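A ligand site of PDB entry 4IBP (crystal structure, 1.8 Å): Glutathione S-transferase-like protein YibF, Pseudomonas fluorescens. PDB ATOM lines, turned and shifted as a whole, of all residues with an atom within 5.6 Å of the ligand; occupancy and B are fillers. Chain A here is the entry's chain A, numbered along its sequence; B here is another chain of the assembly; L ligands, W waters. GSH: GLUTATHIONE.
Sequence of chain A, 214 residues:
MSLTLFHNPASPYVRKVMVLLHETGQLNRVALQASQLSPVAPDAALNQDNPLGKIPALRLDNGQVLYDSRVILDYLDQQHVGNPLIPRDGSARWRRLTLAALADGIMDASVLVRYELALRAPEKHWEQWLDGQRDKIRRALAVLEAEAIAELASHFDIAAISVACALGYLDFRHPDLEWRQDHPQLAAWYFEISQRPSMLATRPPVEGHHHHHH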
ATOM      1  N   SER A  11       0.997 -26.377  12.772  1.00  0.00           N
ATOM      2  CA  SER A  11      -0.171 -26.468  11.899  1.00  0.00           C
ATOM      3  C   SER A  11      -1.254 -27.419  12.387  1.00  0.00           C
ATOM      4  O   SER A  11      -0.992 -28.593  12.667  1.00  0.00           O
ATOM      5  CB  SER A  11       0.260 -26.873  10.486  1.00  0.00           C
ATOM      6  OG  SER A  11      -0.893 -27.094   9.707  1.00  0.00           O
ATOM      7  N   PRO A  12      -2.502 -26.920  12.492  1.00  0.00           N
ATOM      8  CA  PRO A  12      -3.551 -27.816  12.965  1.00  0.00           C
ATOM      9  C   PRO A  12      -4.029 -28.741  11.841  1.00  0.00           C
ATOM     10  O   PRO A  12      -4.573 -29.817  12.126  1.00  0.00           O
ATOM     11  CB  PRO A  12      -4.663 -26.849  13.413  1.00  0.00           C
ATOM     12  CG  PRO A  12      -4.496 -25.660  12.500  1.00  0.00           C
ATOM     13  CD  PRO A  12      -3.001 -25.554  12.232  1.00  0.00           C
ATOM     14  N   TYR A  13      -3.803 -28.370  10.579  1.00  0.00           N
ATOM     15  CA  TYR A  13      -4.194 -29.261   9.494  1.00  0.00           C
ATOM     16  C   TYR A  13      -3.265 -30.454   9.505  1.00  0.00           C
ATOM     17  O   TYR A  13      -3.706 -31.610   9.379  1.00  0.00           O
ATOM     18  CB  TYR A  13      -4.132 -28.550   8.144  1.00  0.00           C
ATOM     19  CG  TYR A  13      -5.011 -27.330   8.043  1.00  0.00           C
ATOM     20  CD1 TYR A  13      -6.356 -27.455   7.682  1.00  0.00           C
ATOM     21  CD2 TYR A  13      -4.514 -26.057   8.290  1.00  0.00           C
ATOM     22  CE1 TYR A  13      -7.172 -26.349   7.582  1.00  0.00           C
ATOM     23  CE2 TYR A  13      -5.316 -24.932   8.182  1.00  0.00           C
ATOM     24  CZ  TYR A  13      -6.649 -25.093   7.826  1.00  0.00           C
ATOM     25  OH  TYR A  13      -7.467 -23.983   7.706  1.00  0.00           O
ATOM     26  N   LYS A  16      -4.119 -32.776  12.432  1.00  0.00           N
ATOM     27  CA  LYS A  16      -5.166 -33.761  12.146  1.00  0.00           C
ATOM     28  C   LYS A  16      -4.559 -35.040  11.582  1.00  0.00           C
ATOM     29  O   LYS A  16      -4.939 -36.135  11.995  1.00  0.00           O
ATOM     30  CB  LYS A  16      -6.200 -33.247  11.128  1.00  0.00           C
ATOM     31  CG  LYS A  16      -7.009 -32.039  11.535  1.00  0.00           C
ATOM     32  CD  LYS A  16      -8.158 -31.785  10.522  1.00  0.00           C
ATOM     33  CE  LYS A  16      -7.605 -31.375   9.183  1.00  0.00           C
ATOM     34  NZ  LYS A  16      -8.725 -31.145   8.206  1.00  0.00           N
ATOM     35  N   LEU A  37       6.824 -21.935   6.305  1.00  0.00           N
ATOM     36  CA  LEU A  37       6.271 -21.224   5.168  1.00  0.00           C
ATOM     37  C   LEU A  37       5.205 -20.224   5.576  1.00  0.00           C
ATOM     38  O   LEU A  37       4.785 -20.173   6.742  1.00  0.00           O
ATOM     39  CB  LEU A  37       5.684 -22.201   4.145  1.00  0.00           C
ATOM     40  CG  LEU A  37       4.768 -23.380   4.543  1.00  0.00           C
ATOM     41  CD1 LEU A  37       3.943 -23.169   5.806  1.00  0.00           C
ATOM     42  CD2 LEU A  37       3.858 -23.673   3.386  1.00  0.00           C
ATOM     43  N   SER A  38       4.769 -19.449   4.591  1.00  0.00           N
ATOM     44  CA  SER A  38       3.653 -18.532   4.740  1.00  0.00           C
ATOM     45  C   SER A  38       3.213 -18.212   3.325  1.00  0.00           C
ATOM     46  O   SER A  38       3.872 -18.607   2.373  1.00  0.00           O
ATOM     47  CB  SER A  38       4.096 -17.265   5.496  1.00  0.00           C
ATOM     48  OG  SER A  38       4.582 -16.285   4.596  1.00  0.00           O
ATOM     49  N   PRO A  39       2.079 -17.509   3.165  1.00  0.00           N
ATOM     50  CA  PRO A  39       1.693 -17.127   1.805  1.00  0.00           C
ATOM     51  C   PRO A  39       2.709 -16.172   1.160  1.00  0.00           C
ATOM     52  O   PRO A  39       2.783 -16.095  -0.068  1.00  0.00           O
ATOM     53  CB  PRO A  39       0.361 -16.404   2.004  1.00  0.00           C
ATOM     54  CG  PRO A  39      -0.182 -16.977   3.271  1.00  0.00           C
ATOM     55  CD  PRO A  39       1.002 -17.236   4.140  1.00  0.00           C
ATOM     56  N   LEU A  52       0.015 -25.551  -4.492  1.00  0.00           N
ATOM     57  CA  LEU A  52      -0.673 -24.534  -3.703  1.00  0.00           C
ATOM     58  C   LEU A  52       0.207 -23.999  -2.573  1.00  0.00           C
ATOM     59  O   LEU A  52      -0.139 -23.014  -1.922  1.00  0.00           O
ATOM     60  CB  LEU A  52      -1.981 -25.094  -3.120  1.00  0.00           C
ATOM     61  CG  LEU A  52      -2.965 -25.663  -4.136  1.00  0.00           C
ATOM     62  CD1 LEU A  52      -4.114 -26.407  -3.436  1.00  0.00           C
ATOM     63  CD2 LEU A  52      -3.522 -24.538  -5.019  1.00  0.00           C
ATOM     64  N   GLY A  53       1.344 -24.648  -2.336  1.00  0.00           N
ATOM     65  CA  GLY A  53       2.250 -24.219  -1.272  1.00  0.00           C
ATOM     66  C   GLY A  53       1.586 -24.253   0.091  1.00  0.00           C
ATOM     67  O   GLY A  53       1.656 -23.275   0.845  1.00  0.00           O
ATOM     68  N   LYS A  54       0.937 -25.373   0.387  1.00  0.00           N
ATOM     69  CA  LYS A  54       0.338 -25.569   1.706  1.00  0.00           C
ATOM     70  C   LYS A  54       0.684 -26.924   2.281  1.00  0.00           C
ATOM     71  O   LYS A  54       0.895 -27.881   1.551  1.00  0.00           O
ATOM     72  CB  LYS A  54      -1.188 -25.442   1.641  1.00  0.00           C
ATOM     73  CG  LYS A  54      -1.667 -24.066   1.240  1.00  0.00           C
ATOM     74  CD  LYS A  54      -3.135 -23.901   1.540  1.00  0.00           C
ATOM     75  CE  LYS A  54      -3.590 -22.497   1.201  1.00  0.00           C
ATOM     76  NZ  LYS A  54      -4.990 -22.293   1.643  1.00  0.00           N
ATOM     77  N   ILE A  55       0.727 -26.993   3.612  1.00  0.00           N
ATOM     78  CA  ILE A  55       0.893 -28.257   4.312  1.00  0.00           C
ATOM     79  C   ILE A  55      -0.407 -28.586   5.064  1.00  0.00           C
ATOM     80  O   ILE A  55      -1.121 -27.681   5.498  1.00  0.00           O
ATOM     81  CB  ILE A  55       2.100 -28.237   5.254  1.00  0.00           C
ATOM     82  CG1 ILE A  55       1.970 -27.149   6.308  1.00  0.00           C
ATOM     83  CG2 ILE A  55       3.391 -28.038   4.466  1.00  0.00           C
ATOM     84  CD1 ILE A  55       3.166 -27.093   7.235  1.00  0.00           C
ATOM     85  N   PRO A  56      -0.699 -29.882   5.254  1.00  0.00           N
ATOM     86  CA  PRO A  56       0.128 -31.049   4.902  1.00  0.00           C
ATOM     87  C   PRO A  56       0.097 -31.365   3.420  1.00  0.00           C
ATOM     88  O   PRO A  56      -0.848 -30.984   2.722  1.00  0.00           O
ATOM     89  CB  PRO A  56      -0.554 -32.185   5.643  1.00  0.00           C
ATOM     90  CG  PRO A  56      -2.027 -31.775   5.621  1.00  0.00           C
ATOM     91  CD  PRO A  56      -1.967 -30.282   5.895  1.00  0.00           C
ATOM     92  N   ASP A  68      -5.529 -31.903  -0.243  1.00  0.00           N
ATOM     93  CA  ASP A  68      -5.109 -31.267   1.001  1.00  0.00           C
ATOM     94  C   ASP A  68      -5.371 -32.215   2.172  1.00  0.00           C
ATOM     95  O   ASP A  68      -5.482 -33.427   1.957  1.00  0.00           O
ATOM     96  CB  ASP A  68      -5.893 -29.960   1.187  1.00  0.00           C
ATOM     97  CG  ASP A  68      -7.424 -30.172   1.181  1.00  0.00           C
ATOM     98  OD1 ASP A  68      -7.889 -31.301   0.960  1.00  0.00           O
ATOM     99  OD2 ASP A  68      -8.162 -29.194   1.383  1.00  0.00           O
ATOM    100  N   SER A  69      -5.485 -31.682   3.378  1.00  0.00           N
ATOM    101  CA  SER A  69      -5.579 -32.524   4.571  1.00  0.00           C
ATOM    102  C   SER A  69      -6.743 -33.529   4.513  1.00  0.00           C
ATOM    103  O   SER A  69      -6.586 -34.703   4.881  1.00  0.00           O
ATOM    104  CB  SER A  69      -5.678 -31.668   5.857  1.00  0.00           C
ATOM    105  OG  SER A  69      -6.833 -30.841   5.866  1.00  0.00           O
ATOM    106  N   ARG A  70      -7.904 -33.081   4.071  1.00  0.00           N
ATOM    107  CA  ARG A  70      -9.065 -33.963   4.017  1.00  0.00           C
ATOM    108  C   ARG A  70      -8.867 -35.145   3.068  1.00  0.00           C
ATOM    109  O   ARG A  70      -9.337 -36.252   3.345  1.00  0.00           O
ATOM    110  CB  ARG A  70     -10.335 -33.202   3.692  1.00  0.00           C
ATOM    111  CG  ARG A  70     -10.860 -32.365   4.842  1.00  0.00           C
ATOM    112  CD  ARG A  70     -12.211 -31.808   4.487  1.00  0.00           C
ATOM    113  NE  ARG A  70     -12.144 -30.427   4.009  1.00  0.00           N
ATOM    114  CZ  ARG A  70     -13.196 -29.725   3.632  1.00  0.00           C
ATOM    115  NH1 ARG A  70     -14.396 -30.287   3.641  1.00  0.00           N
ATOM    116  NH2 ARG A  70     -13.045 -28.479   3.222  1.00  0.00           N
ATOM    117  N   ASP A 104     -12.700 -27.534  10.054  1.00  0.00           N
ATOM    118  CA  ASP A 104     -11.825 -26.950   9.049  1.00  0.00           C
ATOM    119  C   ASP A 104     -12.121 -25.468   8.820  1.00  0.00           C
ATOM    120  O   ASP A 104     -11.199 -24.680   8.635  1.00  0.00           O
ATOM    121  CB  ASP A 104     -11.912 -27.704   7.708  1.00  0.00           C
ATOM    122  CG  ASP A 104     -11.224 -29.059   7.745  1.00  0.00           C
ATOM    123  OD1 ASP A 104     -10.561 -29.370   8.753  1.00  0.00           O
ATOM    124  OD2 ASP A 104     -11.349 -29.819   6.759  1.00  0.00           O
ATOM    125  N   ASP A 108      -9.673 -22.406   9.061  1.00  0.00           N
ATOM    126  CA  ASP A 108      -9.496 -21.510   7.919  1.00  0.00           C
ATOM    127  C   ASP A 108      -9.540 -20.048   8.378  1.00  0.00           C
ATOM    128  O   ASP A 108      -8.703 -19.237   8.010  1.00  0.00           O
ATOM    129  CB  ASP A 108     -10.590 -21.718   6.865  1.00  0.00           C
ATOM    130  CG  ASP A 108     -10.520 -23.078   6.175  1.00  0.00           C
ATOM    131  OD1 ASP A 108      -9.497 -23.785   6.281  1.00  0.00           O
ATOM    132  OD2 ASP A 108     -11.513 -23.429   5.490  1.00  0.00           O
ATOM    133  N   VAL A 111      -6.592 -19.136  10.841  1.00  0.00           N
ATOM    134  CA  VAL A 111      -5.349 -18.939  10.106  1.00  0.00           C
ATOM    135  C   VAL A 111      -5.347 -17.613   9.343  1.00  0.00           C
ATOM    136  O   VAL A 111      -4.316 -16.935   9.299  1.00  0.00           O
ATOM    137  CB  VAL A 111      -5.049 -20.144   9.188  1.00  0.00           C
ATOM    138  CG1 VAL A 111      -3.987 -19.822   8.178  1.00  0.00           C
ATOM    139  CG2 VAL A 111      -4.644 -21.344  10.021  1.00  0.00           C
ATOM    140  N   TYR A 115      -2.493 -14.628   9.982  1.00  0.00           N
ATOM    141  CA  TYR A 115      -1.648 -14.061   8.926  1.00  0.00           C
ATOM    142  C   TYR A 115      -1.771 -12.542   8.862  1.00  0.00           C
ATOM    143  O   TYR A 115      -0.801 -11.827   8.634  1.00  0.00           O
ATOM    144  CB  TYR A 115      -2.004 -14.650   7.563  1.00  0.00           C
ATOM    145  CG  TYR A 115      -1.537 -16.074   7.363  1.00  0.00           C
ATOM    146  CD1 TYR A 115      -0.516 -16.590   8.150  1.00  0.00           C
ATOM    147  CD2 TYR A 115      -2.114 -16.893   6.410  1.00  0.00           C
ATOM    148  CE1 TYR A 115      -0.081 -17.883   7.989  1.00  0.00           C
ATOM    149  CE2 TYR A 115      -1.683 -18.194   6.239  1.00  0.00           C
ATOM    150  CZ  TYR A 115      -0.663 -18.680   7.029  1.00  0.00           C
ATOM    151  OH  TYR A 115      -0.215 -19.967   6.878  1.00  0.00           O
ATOM    152  N   ARG B  70     -17.260 -29.824  -0.958  1.00  0.00           N
ATOM    153  CA  ARG B  70     -16.760 -31.176  -1.141  1.00  0.00           C
ATOM    154  C   ARG B  70     -17.609 -32.229  -0.428  1.00  0.00           C
ATOM    155  O   ARG B  70     -17.774 -33.341  -0.941  1.00  0.00           O
ATOM    156  CB  ARG B  70     -15.291 -31.289  -0.748  1.00  0.00           C
ATOM    157  CG  ARG B  70     -14.347 -30.653  -1.741  1.00  0.00           C
ATOM    158  CD  ARG B  70     -12.919 -30.983  -1.362  1.00  0.00           C
ATOM    159  NE  ARG B  70     -12.279 -29.897  -0.623  1.00  0.00           N
ATOM    160  CZ  ARG B  70     -11.028 -29.953  -0.177  1.00  0.00           C
ATOM    161  NH1 ARG B  70     -10.312 -31.052  -0.363  1.00  0.00           N
ATOM    162  NH2 ARG B  70     -10.517 -28.925   0.473  1.00  0.00           N
ATOM    163  N   ASP B 108      -9.821 -20.992  -3.882  1.00  0.00           N
ATOM    164  CA  ASP B 108      -9.549 -20.382  -2.582  1.00  0.00           C
ATOM    165  C   ASP B 108      -8.709 -19.112  -2.751  1.00  0.00           C
ATOM    166  O   ASP B 108      -9.015 -18.067  -2.186  1.00  0.00           O
ATOM    167  CB  ASP B 108      -8.793 -21.339  -1.651  1.00  0.00           C
ATOM    168  CG  ASP B 108      -9.615 -22.558  -1.234  1.00  0.00           C
ATOM    169  OD1 ASP B 108     -10.849 -22.577  -1.417  1.00  0.00           O
ATOM    170  OD2 ASP B 108      -9.010 -23.504  -0.686  1.00  0.00           O
ATOM    171  N   GLN B 133      -0.874 -15.097  -3.487  1.00  0.00           N
ATOM    172  CA  GLN B 133      -2.071 -15.838  -3.874  1.00  0.00           C
ATOM    173  C   GLN B 133      -2.075 -16.128  -5.374  1.00  0.00           C
ATOM    174  O   GLN B 133      -2.349 -17.250  -5.790  1.00  0.00           O
ATOM    175  CB  GLN B 133      -3.329 -15.090  -3.424  1.00  0.00           C
ATOM    176  CG  GLN B 133      -3.424 -14.941  -1.904  1.00  0.00           C
ATOM    177  CD  GLN B 133      -3.470 -16.290  -1.191  1.00  0.00           C
ATOM    178  OE1 GLN B 133      -4.104 -17.229  -1.660  1.00  0.00           O
ATOM    179  NE2 GLN B 133      -2.793 -16.378  -0.045  1.00  0.00           N
ATOM    180  N   LYS B 136       0.146 -19.148  -6.294  1.00  0.00           N
ATOM    181  CA  LYS B 136      -0.485 -20.461  -6.104  1.00  0.00           C
ATOM    182  C   LYS B 136      -1.288 -20.829  -7.339  1.00  0.00           C
ATOM    183  O   LYS B 136      -1.148 -21.922  -7.879  1.00  0.00           O
ATOM    184  CB  LYS B 136      -1.390 -20.453  -4.871  1.00  0.00           C
ATOM    185  CG  LYS B 136      -0.697 -20.135  -3.554  1.00  0.00           C
ATOM    186  CD  LYS B 136      -1.686 -20.212  -2.387  1.00  0.00           C
ATOM    187  CE  LYS B 136      -1.073 -19.733  -1.075  1.00  0.00           C
ATOM    188  NZ  LYS B 136       0.112 -20.531  -0.658  1.00  0.00           N
HETATM  189  N1  GSH L   1      -7.050 -26.733   2.769  1.00  0.00           N
HETATM  190  CA1 GSH L   1      -5.759 -26.978   3.309  1.00  0.00           C
HETATM  191  C1  GSH L   1      -5.780 -28.241   4.122  1.00  0.00           C
HETATM  192  O11 GSH L   1      -6.858 -28.633   4.659  1.00  0.00           O
HETATM  193  O12 GSH L   1      -4.741 -28.947   4.277  1.00  0.00           O
HETATM  194  CB1 GSH L   1      -5.358 -25.825   4.174  1.00  0.00           C
HETATM  195  CG1 GSH L   1      -3.946 -26.084   4.714  1.00  0.00           C
HETATM  196  CD1 GSH L   1      -3.268 -24.817   5.222  1.00  0.00           C
HETATM  197  OE1 GSH L   1      -3.773 -23.732   5.058  1.00  0.00           O
HETATM  198  N2  GSH L   1      -1.973 -24.924   5.930  1.00  0.00           N
HETATM  199  CA2 GSH L   1      -1.287 -23.760   6.394  1.00  0.00           C
HETATM  200  C2  GSH L   1      -0.366 -23.343   5.264  1.00  0.00           C
HETATM  201  O2  GSH L   1       0.162 -24.218   4.563  1.00  0.00           O
HETATM  202  CB2 GSH L   1      -0.394 -24.150   7.528  1.00  0.00           C
HETATM  203  SG2 GSH L   1      -1.369 -24.252   8.994  1.00  0.00           S
HETATM  204  N3  GSH L   1      -0.089 -21.947   4.965  1.00  0.00           N
HETATM  205  CA3 GSH L   1       0.797 -21.628   3.866  1.00  0.00           C
HETATM  206  C3  GSH L   1       0.038 -20.809   2.867  1.00  0.00           C
HETATM  207  O31 GSH L   1       0.629 -20.311   1.870  1.00  0.00           O
HETATM  208  O32 GSH L   1      -1.196 -20.613   3.025  1.00  0.00           O
HETATM  209  O   HOH W   1      -3.320 -18.515   1.904  1.00  0.00           O
HETATM  210  O   HOH W   2      -5.707 -26.223  -0.004  1.00  0.00           O
HETATM  211  O   HOH W   3      -2.810 -28.758   2.324  1.00  0.00           O
HETATM  212  O   HOH W   4       3.236 -21.022   0.830  1.00  0.00           O
HETATM  213  O   HOH W   5      -0.675 -21.178   9.393  1.00  0.00           O
HETATM  214  O   HOH W   6      -6.435 -22.376   5.415  1.00  0.00           O
HETATM  215  O   HOH W   7      -3.282 -21.175   4.275  1.00  0.00           O
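The backbone nitrogen (N) of Pro 39 sits close to an oxygen (O31) of the ligand.
O of Gly 53 sits close to O31 of the ligand (3.3 Å).
Pro 12 touches the ligand.
CD1 of Tyr 13 touches O11 of the ligand, at 3.3 Å.
Leu 37 touches the ligand.
C of Ser 38 touches O31 of the ligand, at 3.6 Å.
Lys 54 touches the ligand.
CD of Pro 56 touches O12 of the ligand, 3.5 Å away.
The side-chain carboxylate (OD2) of Asp 68 is in salt-bridge range of a nitrogen (N1) of the ligand, at 3.0 Å.
The side-chain amino group of Lys 136 of chain B lies within salt-bridge range of an oxygen (O31) of the ligand, 2.6 Å away.
An oxygen (O11) of the ligand is in hydrogen-bond range of the side-chain hydroxyl of Ser 69 (2.5 Å).
N3 of the ligand lies within hydrogen-bond range of OH of Tyr 115 (2.8 Å).
N of Ser 69 sits at hydrogen-bond distance from O12 of the ligand (3.0 Å).
OG of Ser 11 sits close to SG2 of the ligand, at 3.0 Å.
The backbone NH (N) of Ile 55 sits at hydrogen-bond distance from an oxygen (O2) of the ligand, at 3.0 Å.
N2 of the ligand is in hydrogen-bond range of O of Ile 55 (2.9 Å).
Water W7 bridges an oxygen (O32) of the ligand (2.5 Å) and the side-chain amino group (NZ) of Lys 54 (3.3 Å).
Water W3 bridges O12 of the ligand and O of Pro 56.
Water W4 lies within hydrogen-bond range of O of Gly 53 (2.8 Å), O31 of the ligand (2.9 Å), O of Ser 38 (2.9 Å) and NZ of Lys 136 of chain B (3.5 Å).
Water W6 lies within hydrogen-bond range of OH of Tyr 13 (3.0 Å), OE1 of the ligand (3.0 Å) and OD1 of Asp 108 of chain A (3.5 Å).
Water W5 bridges OH of Tyr 115 (2.8 Å) and SG2 of the ligand (3.2 Å).
Water W1 bridges the side-chain amide nitrogen of Gln 133 of chain B (2.9 Å) and an oxygen (O32) of the ligand (3.2 Å).
The side-chain amino group of Lys 16 is in hydrogen-bond range of the side-chain hydroxyl of Ser 69 (3.0 Å).
O of Gly 53 lies within hydrogen-bond range of NZ of Lys 136 of chain B, 3.5 Å away.
The guanidinium group of Arg 70 of chain B is in salt-bridge range of the side-chain carboxylate of Asp 68 (2.5 Å).
OG of Ser 11 sits close to N of Tyr 13, 3.3 Å away.
The backbone carbonyl oxygen (O) of Leu 52 sits at hydrogen-bond distance from the side-chain amino group (NZ) of Lys 136 of chain B (2.8 Å).
The side-chain carboxylate of Asp 108 of chain A lies within hydrogen-bond range of the side-chain hydroxyl of Tyr 13, at 2.5 Å.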
